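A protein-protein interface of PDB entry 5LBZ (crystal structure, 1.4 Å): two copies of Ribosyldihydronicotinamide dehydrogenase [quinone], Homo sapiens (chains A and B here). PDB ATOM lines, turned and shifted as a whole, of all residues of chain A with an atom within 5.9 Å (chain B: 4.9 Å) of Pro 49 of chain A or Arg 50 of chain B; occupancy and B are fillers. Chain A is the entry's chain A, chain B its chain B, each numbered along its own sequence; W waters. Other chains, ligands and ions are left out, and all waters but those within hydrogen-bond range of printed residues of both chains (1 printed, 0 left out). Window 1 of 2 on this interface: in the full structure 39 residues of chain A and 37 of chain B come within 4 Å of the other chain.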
ATOM      1  N   TYR A  43      -8.997 -31.004  26.721  1.00  0.00           N
ATOM      2  CA  TYR A  43      -9.717 -29.768  27.009  1.00  0.00           C
ATOM      3  C   TYR A  43     -10.293 -29.750  28.424  1.00  0.00           C
ATOM      4  O   TYR A  43     -10.269 -28.716  29.081  1.00  0.00           O
ATOM      5  CB  TYR A  43     -10.839 -29.513  26.004  1.00  0.00           C
ATOM      6  CG  TYR A  43     -10.351 -29.111  24.637  1.00  0.00           C
ATOM      7  CD1 TYR A  43      -9.921 -27.823  24.369  1.00  0.00           C
ATOM      8  CD2 TYR A  43     -10.326 -30.016  23.597  1.00  0.00           C
ATOM      9  CE1 TYR A  43      -9.501 -27.450  23.085  1.00  0.00           C
ATOM     10  CE2 TYR A  43      -9.922 -29.660  22.313  1.00  0.00           C
ATOM     11  CZ  TYR A  43      -9.530 -28.377  22.064  1.00  0.00           C
ATOM     12  OH  TYR A  43      -9.142 -28.035  20.780  1.00  0.00           O
ATOM     13  N   ASN A  46      -7.745 -28.892  30.752  1.00  0.00           N
ATOM     14  CA  ASN A  46      -7.203 -27.592  30.422  1.00  0.00           C
ATOM     15  C   ASN A  46      -5.686 -27.691  30.228  1.00  0.00           C
ATOM     16  O   ASN A  46      -4.918 -26.861  30.665  1.00  0.00           O
ATOM     17  CB  ASN A  46      -7.566 -26.533  31.462  1.00  0.00           C
ATOM     18  CG  ASN A  46      -7.343 -25.143  30.934  1.00  0.00           C
ATOM     19  OD1 ASN A  46      -7.598 -24.867  29.728  1.00  0.00           O
ATOM     20  ND2 ASN A  46      -6.854 -24.276  31.774  1.00  0.00           N
ATOM     21  N   LEU A  47      -5.262 -28.714  29.492  1.00  0.00           N
ATOM     22  CA  LEU A  47      -3.848 -28.974  29.338  1.00  0.00           C
ATOM     23  C   LEU A  47      -3.119 -27.747  28.800  1.00  0.00           C
ATOM     24  O   LEU A  47      -3.531 -27.173  27.782  1.00  0.00           O
ATOM     25  CB  LEU A  47      -3.625 -30.144  28.387  1.00  0.00           C
ATOM     26  CG  LEU A  47      -2.183 -30.613  28.296  1.00  0.00           C
ATOM     27  CD1 LEU A  47      -1.883 -31.634  29.385  1.00  0.00           C
ATOM     28  CD2 LEU A  47      -1.884 -31.209  26.925  1.00  0.00           C
ATOM     29  N   GLU A  48      -1.991 -27.406  29.426  1.00  0.00           N
ATOM     30  CA  GLU A  48      -1.130 -26.322  28.958  1.00  0.00           C
ATOM     31  C   GLU A  48      -0.485 -26.789  27.628  1.00  0.00           C
ATOM     32  O   GLU A  48       0.172 -27.807  27.578  1.00  0.00           O
ATOM     33  CB  GLU A  48      -0.054 -26.027  29.981  1.00  0.00           C
ATOM     34  CG  GLU A  48       1.056 -25.105  29.472  1.00  0.00           C
ATOM     35  CD  GLU A  48       0.560 -23.711  29.228  1.00  0.00           C
ATOM     36  OE1 GLU A  48       0.174 -23.058  30.232  1.00  0.00           O
ATOM     37  OE2 GLU A  48       0.490 -23.315  28.064  1.00  0.00           O
ATOM     38  N   PRO A  49      -0.643 -25.980  26.539  1.00  0.00           N
ATOM     39  CA  PRO A  49       0.010 -26.388  25.296  1.00  0.00           C
ATOM     40  C   PRO A  49       1.365 -25.767  25.044  1.00  0.00           C
ATOM     41  O   PRO A  49       2.111 -26.249  24.200  1.00  0.00           O
ATOM     42  CB  PRO A  49      -0.969 -25.946  24.215  1.00  0.00           C
ATOM     43  CG  PRO A  49      -2.241 -25.641  24.935  1.00  0.00           C
ATOM     44  CD  PRO A  49      -1.829 -25.164  26.284  1.00  0.00           C
ATOM     45  N   ARG A  50       1.652 -24.648  25.735  1.00  0.00           N
ATOM     46  CA  ARG A  50       2.858 -23.874  25.449  1.00  0.00           C
ATOM     47  C   ARG A  50       4.075 -24.520  26.055  1.00  0.00           C
ATOM     48  O   ARG A  50       4.045 -24.984  27.180  1.00  0.00           O
ATOM     49  CB  ARG A  50       2.724 -22.468  26.012  1.00  0.00           C
ATOM     50  CG  ARG A  50       1.526 -21.692  25.531  1.00  0.00           C
ATOM     51  CD  ARG A  50       1.467 -20.388  26.305  1.00  0.00           C
ATOM     52  NE  ARG A  50       0.209 -19.651  26.257  1.00  0.00           N
ATOM     53  CZ  ARG A  50      -0.808 -19.768  27.118  1.00  0.00           C
ATOM     54  NH1 ARG A  50      -0.895 -20.735  27.983  1.00  0.00           N
ATOM     55  NH2 ARG A  50      -1.795 -18.928  27.034  1.00  0.00           N
ATOM     56  N   ALA A  51       5.182 -24.508  25.315  1.00  0.00           N
ATOM     57  CA  ALA A  51       6.456 -25.025  25.798  1.00  0.00           C
ATOM     58  C   ALA A  51       7.163 -23.863  26.502  1.00  0.00           C
ATOM     59  O   ALA A  51       7.723 -22.993  25.841  1.00  0.00           O
ATOM     60  CB  ALA A  51       7.283 -25.531  24.637  1.00  0.00           C
ATOM     61  N   ALA A 111      -4.141 -27.576  18.347  1.00  0.00           N
ATOM     62  CA  ALA A 111      -2.990 -27.105  19.111  1.00  0.00           C
ATOM     63  C   ALA A 111      -2.878 -27.723  20.494  1.00  0.00           C
ATOM     64  O   ALA A 111      -1.762 -27.911  20.968  1.00  0.00           O
ATOM     65  CB  ALA A 111      -3.003 -25.580  19.211  1.00  0.00           C
ATOM     66  N   ILE A 112      -3.990 -27.970  21.181  1.00  0.00           N
ATOM     67  CA  ILE A 112      -3.878 -28.517  22.523  1.00  0.00           C
ATOM     68  C   ILE A 112      -3.159 -29.891  22.482  1.00  0.00           C
ATOM     69  O   ILE A 112      -2.415 -30.252  23.378  1.00  0.00           O
ATOM     70  CB  ILE A 112      -5.243 -28.568  23.248  1.00  0.00           C
ATOM     71  CG1 ILE A 112      -5.055 -28.792  24.758  1.00  0.00           C
ATOM     72  CG2 ILE A 112      -6.191 -29.599  22.638  1.00  0.00           C
ATOM     73  CD1 ILE A 112      -6.329 -28.606  25.572  1.00  0.00           C
ATOM     74  N   LYS A 114      -1.136 -30.837  19.904  1.00  0.00           N
ATOM     75  CA  LYS A 114       0.229 -30.555  19.535  1.00  0.00           C
ATOM     76  C   LYS A 114       1.053 -30.261  20.796  1.00  0.00           C
ATOM     77  O   LYS A 114       2.196 -30.663  20.903  1.00  0.00           O
ATOM     78  CB  LYS A 114       0.336 -29.376  18.580  1.00  0.00           C
ATOM     79  CG  LYS A 114       1.733 -29.159  18.029  1.00  0.00           C
ATOM     80  CD  LYS A 114       2.318 -30.447  17.449  1.00  0.00           C
ATOM     81  CE  LYS A 114       3.501 -30.188  16.514  1.00  0.00           C
ATOM     82  NZ  LYS A 114       4.596 -29.388  17.166  1.00  0.00           N
ATOM     83  N   GLY A 115       0.460 -29.517  21.733  1.00  0.00           N
ATOM     84  CA  GLY A 115       1.143 -29.203  22.962  1.00  0.00           C
ATOM     85  C   GLY A 115       1.427 -30.422  23.810  1.00  0.00           C
ATOM     86  O   GLY A 115       2.502 -30.520  24.433  1.00  0.00           O
ATOM     87  N   TRP A 116       0.495 -31.366  23.856  1.00  0.00           N
ATOM     88  CA  TRP A 116       0.738 -32.650  24.501  1.00  0.00           C
ATOM     89  C   TRP A 116       1.974 -33.295  23.890  1.00  0.00           C
ATOM     90  O   TRP A 116       2.870 -33.747  24.604  1.00  0.00           O
ATOM     91  CB  TRP A 116      -0.487 -33.540  24.414  1.00  0.00           C
ATOM     92  CG  TRP A 116      -0.431 -34.831  25.151  1.00  0.00           C
ATOM     93  CD1 TRP A 116      -1.009 -35.095  26.357  1.00  0.00           C
ATOM     94  CD2 TRP A 116       0.144 -36.065  24.708  1.00  0.00           C
ATOM     95  NE1 TRP A 116      -0.804 -36.393  26.702  1.00  0.00           N
ATOM     96  CE2 TRP A 116      -0.108 -37.022  25.713  1.00  0.00           C
ATOM     97  CE3 TRP A 116       0.850 -36.462  23.563  1.00  0.00           C
ATOM     98  CZ2 TRP A 116       0.365 -38.319  25.622  1.00  0.00           C
ATOM     99  CZ3 TRP A 116       1.312 -37.749  23.483  1.00  0.00           C
ATOM    100  CH2 TRP A 116       1.056 -38.658  24.509  1.00  0.00           C
ATOM    101  N   ASP A 118       4.477 -31.920  22.154  1.00  0.00           N
ATOM    102  CA  ASP A 118       5.650 -31.098  22.382  1.00  0.00           C
ATOM    103  C   ASP A 118       6.181 -31.246  23.797  1.00  0.00           C
ATOM    104  O   ASP A 118       7.397 -31.265  24.009  1.00  0.00           O
ATOM    105  CB  ASP A 118       5.331 -29.611  22.183  1.00  0.00           C
ATOM    106  CG  ASP A 118       5.002 -29.207  20.757  1.00  0.00           C
ATOM    107  OD1 ASP A 118       5.241 -29.995  19.814  1.00  0.00           O
ATOM    108  OD2 ASP A 118       4.510 -28.076  20.545  1.00  0.00           O
ATOM    109  N   ARG A 119       5.276 -31.295  24.775  1.00  0.00           N
ATOM    110  CA  ARG A 119       5.676 -31.243  26.180  1.00  0.00           C
ATOM    111  C   ARG A 119       5.874 -32.634  26.789  1.00  0.00           C
ATOM    112  O   ARG A 119       6.740 -32.811  27.647  1.00  0.00           O
ATOM    113  CB  ARG A 119       4.619 -30.486  26.965  1.00  0.00           C
ATOM    114  CG  ARG A 119       4.456 -29.042  26.539  1.00  0.00           C
ATOM    115  CD  ARG A 119       3.313 -28.346  27.243  1.00  0.00           C
ATOM    116  NE  ARG A 119       3.565 -28.122  28.656  1.00  0.00           N
ATOM    117  CZ  ARG A 119       2.865 -28.618  29.681  1.00  0.00           C
ATOM    118  NH1 ARG A 119       1.792 -29.365  29.465  1.00  0.00           N
ATOM    119  NH2 ARG A 119       3.274 -28.411  30.921  1.00  0.00           N
ATOM    120  N   GLU B  48      -2.927 -17.519  23.884  1.00  0.00           N
ATOM    121  CA  GLU B  48      -3.750 -18.689  24.135  1.00  0.00           C
ATOM    122  C   GLU B  48      -3.745 -19.607  22.912  1.00  0.00           C
ATOM    123  O   GLU B  48      -4.101 -19.204  21.835  1.00  0.00           O
ATOM    124  CB  GLU B  48      -5.189 -18.243  24.401  1.00  0.00           C
ATOM    125  CG  GLU B  48      -6.197 -19.390  24.493  1.00  0.00           C
ATOM    126  CD  GLU B  48      -5.945 -20.271  25.664  1.00  0.00           C
ATOM    127  OE1 GLU B  48      -6.162 -19.808  26.783  1.00  0.00           O
ATOM    128  OE2 GLU B  48      -5.526 -21.427  25.483  1.00  0.00           O
ATOM    129  N   PRO B  49      -3.330 -20.894  23.084  1.00  0.00           N
ATOM    130  CA  PRO B  49      -3.360 -21.776  21.919  1.00  0.00           C
ATOM    131  C   PRO B  49      -4.595 -22.609  21.778  1.00  0.00           C
ATOM    132  O   PRO B  49      -4.852 -23.159  20.703  1.00  0.00           O
ATOM    133  CB  PRO B  49      -2.142 -22.690  22.137  1.00  0.00           C
ATOM    134  CG  PRO B  49      -1.347 -22.037  23.215  1.00  0.00           C
ATOM    135  CD  PRO B  49      -2.352 -21.338  24.087  1.00  0.00           C
ATOM    136  N   ARG B  50      -5.347 -22.764  22.871  1.00  0.00           N
ATOM    137  CA  ARG B  50      -6.484 -23.680  22.866  1.00  0.00           C
ATOM    138  C   ARG B  50      -7.695 -23.084  22.153  1.00  0.00           C
ATOM    139  O   ARG B  50      -8.003 -21.914  22.362  1.00  0.00           O
ATOM    140  CB  ARG B  50      -6.891 -24.018  24.299  1.00  0.00           C
ATOM    141  CG  ARG B  50      -5.786 -24.587  25.171  1.00  0.00           C
ATOM    142  CD  ARG B  50      -6.303 -24.715  26.580  1.00  0.00           C
ATOM    143  NE  ARG B  50      -5.318 -24.910  27.621  1.00  0.00           N
ATOM    144  CZ  ARG B  50      -4.714 -23.964  28.339  1.00  0.00           C
ATOM    145  NH1 ARG B  50      -4.858 -22.671  28.066  1.00  0.00           N
ATOM    146  NH2 ARG B  50      -3.978 -24.321  29.368  1.00  0.00           N
ATOM    147  N   ALA B  51      -8.382 -23.903  21.369  1.00  0.00           N
ATOM    148  CA  ALA B  51      -9.597 -23.477  20.697  1.00  0.00           C
ATOM    149  C   ALA B  51     -10.774 -23.737  21.646  1.00  0.00           C
ATOM    150  O   ALA B  51     -11.187 -24.874  21.800  1.00  0.00           O
ATOM    151  CB  ALA B  51      -9.767 -24.248  19.383  1.00  0.00           C
ATOM    152  N   THR B  52     -11.248 -22.685  22.322  1.00  0.00           N
ATOM    153  CA  THR B  52     -12.315 -22.865  23.303  1.00  0.00           C
ATOM    154  C   THR B  52     -13.388 -21.836  23.152  1.00  0.00           C
ATOM    155  O   THR B  52     -13.232 -20.853  22.438  1.00  0.00           O
ATOM    156  CB  THR B  52     -11.774 -22.861  24.753  1.00  0.00           C
ATOM    157  OG1 THR B  52     -11.594 -21.513  25.207  1.00  0.00           O
ATOM    158  CG2 THR B  52     -10.504 -23.693  24.906  1.00  0.00           C
ATOM    159  N   ASP B  55     -13.071 -17.983  23.161  1.00  0.00           N
ATOM    160  CA  ASP B  55     -12.770 -17.222  21.949  1.00  0.00           C
ATOM    161  C   ASP B  55     -13.941 -16.418  21.396  1.00  0.00           C
ATOM    162  O   ASP B  55     -13.756 -15.579  20.515  1.00  0.00           O
ATOM    163  CB  ASP B  55     -12.203 -18.167  20.885  1.00  0.00           C
ATOM    164  CG  ASP B  55     -10.868 -18.762  21.285  1.00  0.00           C
ATOM    165  OD1 ASP B  55     -10.293 -18.299  22.283  1.00  0.00           O
ATOM    166  OD2 ASP B  55     -10.399 -19.698  20.597  1.00  0.00           O
ATOM    167  N   ALA B 111       3.319 -25.707  19.330  1.00  0.00           N
ATOM    168  CA  ALA B 111       1.885 -25.631  19.628  1.00  0.00           C
ATOM    169  C   ALA B 111       1.352 -24.204  19.730  1.00  0.00           C
ATOM    170  O   ALA B 111       0.212 -23.945  19.352  1.00  0.00           O
ATOM    171  CB  ALA B 111       1.542 -26.394  20.879  1.00  0.00           C
ATOM    172  N   ARG B 119      -6.888 -20.478  15.721  1.00  0.00           N
ATOM    173  CA  ARG B 119      -7.786 -19.473  16.282  1.00  0.00           C
ATOM    174  C   ARG B 119      -7.902 -18.248  15.377  1.00  0.00           C
ATOM    175  O   ARG B 119      -8.990 -17.627  15.310  1.00  0.00           O
ATOM    176  CB  ARG B 119      -7.286 -19.066  17.660  1.00  0.00           C
ATOM    177  CG  ARG B 119      -7.303 -20.206  18.674  1.00  0.00           C
ATOM    178  CD  ARG B 119      -6.665 -19.796  19.993  1.00  0.00           C
ATOM    179  NE  ARG B 119      -7.478 -18.850  20.749  1.00  0.00           N
ATOM    180  CZ  ARG B 119      -7.120 -17.622  21.119  1.00  0.00           C
ATOM    181  NH1 ARG B 119      -5.895 -17.176  20.865  1.00  0.00           N
ATOM    182  NH2 ARG B 119      -7.995 -16.840  21.729  1.00  0.00           N
HETATM  183  O   HOH W   1      -6.660 -26.688  20.706  1.00  0.00           O
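Ala 51 of chain B touches Tyr 43 of chain A (O to CE1, 3.3 Å).
Arg 50 of chain B touches Glu 48 of chain A (NH2 to CA, 3.5 Å).
Pro 49 of chain A touches Arg 50 of chain B.
Pro 49 of chain A touches Ala 111 of chain B (O to CB, 3.4 Å).
Arg 50 of chain A touches Glu 48 of chain B (NH2 to CA, 3.5 Å).
Pro 49 of chain B touches Arg 50 of chain A (CG to CG, 3.7 Å).
Ala 111 of chain A touches Pro 49 of chain B.
Ala 111 of chain A touches Ala 111 of chain B (CB to O, 3.6 Å).
Lys 114 of chain A touches Ala 111 of chain B (CG to CA, 3.9 Å).
Ala 111 of chain B touches Gly 115 of chain A.
Glu 48 of chain A touches Arg 50 of chain B, and with the chains exchanged Arg 50 of chain A touches Glu 48 of chain B.
Pro 49 of chain A touches Arg 50 of chain B, and with the chains exchanged Arg 50 of chain A touches Pro 49 of chain B.
Pro 49 of chain A touches Ala 111 of chain B, and with the chains exchanged Ala 111 of chain A touches Pro 49 of chain B.
Ala 111 of chain A touches its own counterpart, Ala 111 of chain B.
NZ of Lys 114 of chain A is in salt-bridge range of OD1 of Asp 118 of chain A, at 2.8 Å.
The side-chain carboxylate (OE2) of Glu 48 of chain B lies within salt-bridge range of the guanidinium group (NH1) of Arg 50 of chain B, 2.9 Å away.
O of Glu 48 of chain A sits at hydrogen-bond distance from NH1 of Arg 119 of chain A (2.9 Å).
NH1 of Arg 119 of chain B is in hydrogen-bond range of O of Glu 48 of chain B (2.9 Å).
The side-chain carboxylate of Glu 48 of chain A is in salt-bridge range of the guanidinium group of Arg 50 of chain A.
The backbone carbonyl oxygen of Leu 47 of chain A sits at hydrogen-bond distance from the guanidinium group of Arg 50 of chain B.
OD2 of Asp 118 of chain A is in hydrogen-bond range of N of Ala 111 of chain B, at 2.9 Å.
NH2 of Arg 50 of chain B is in hydrogen-bond range of O of Asn 46 of chain A (3.0 Å).
Printed residues of chain B within 4 Å of Leu 47 of chain A: Arg 50.
Printed residues of chain B within 4 Å of Glu 48 of chain A: Arg 50 (3.5 Å).
Arg 119 of chain A touches none of the printed residues of chain B.
Of the printed residues of chain A, Pro 49 of chain B touches Arg 50 and Ala 111.
Of the printed residues of chain A, Arg 50 of chain B touches Asn 46, Leu 47, Glu 48 and Pro 49.
Of the printed residues of chain A, Ala 111 of chain B touches Pro 49, Ala 111, Lys 114, Gly 115 and Asp 118.
The nearest residue of chain B that does not touch Pro 49 of chain A is Pro 49 of chain B (4.04 Å).
The nearest printed residue of chain A that does not touch Glu 48 of chain B is Pro 49 of chain A (5.3 Å).
Water W1 lies within hydrogen-bond range of OH of Tyr 43 of chain A (2.8 Å), N of Ile 112 of chain A (3.0 Å) and N of Ala 51 of chain B (3.3 Å).
Of the 8 printed residues of chain B, 5 touch a printed residue of chain A.
Hydrophobic or aromatic side chains of chain B that line the printed part of chain A: Pro 49 and Ala 111.
Hydrophobic or aromatic side chains of chain A that line the printed part of chain B: Tyr 43, Pro 49 and Ala 111.
Along chain A the printed residues that touch a printed residue of chain B span positions 43 to 118.
Among the printed residues, no Asp or Glu carboxylate lies within 4 Å of a Lys or Arg side-chain nitrogen of the other chain.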
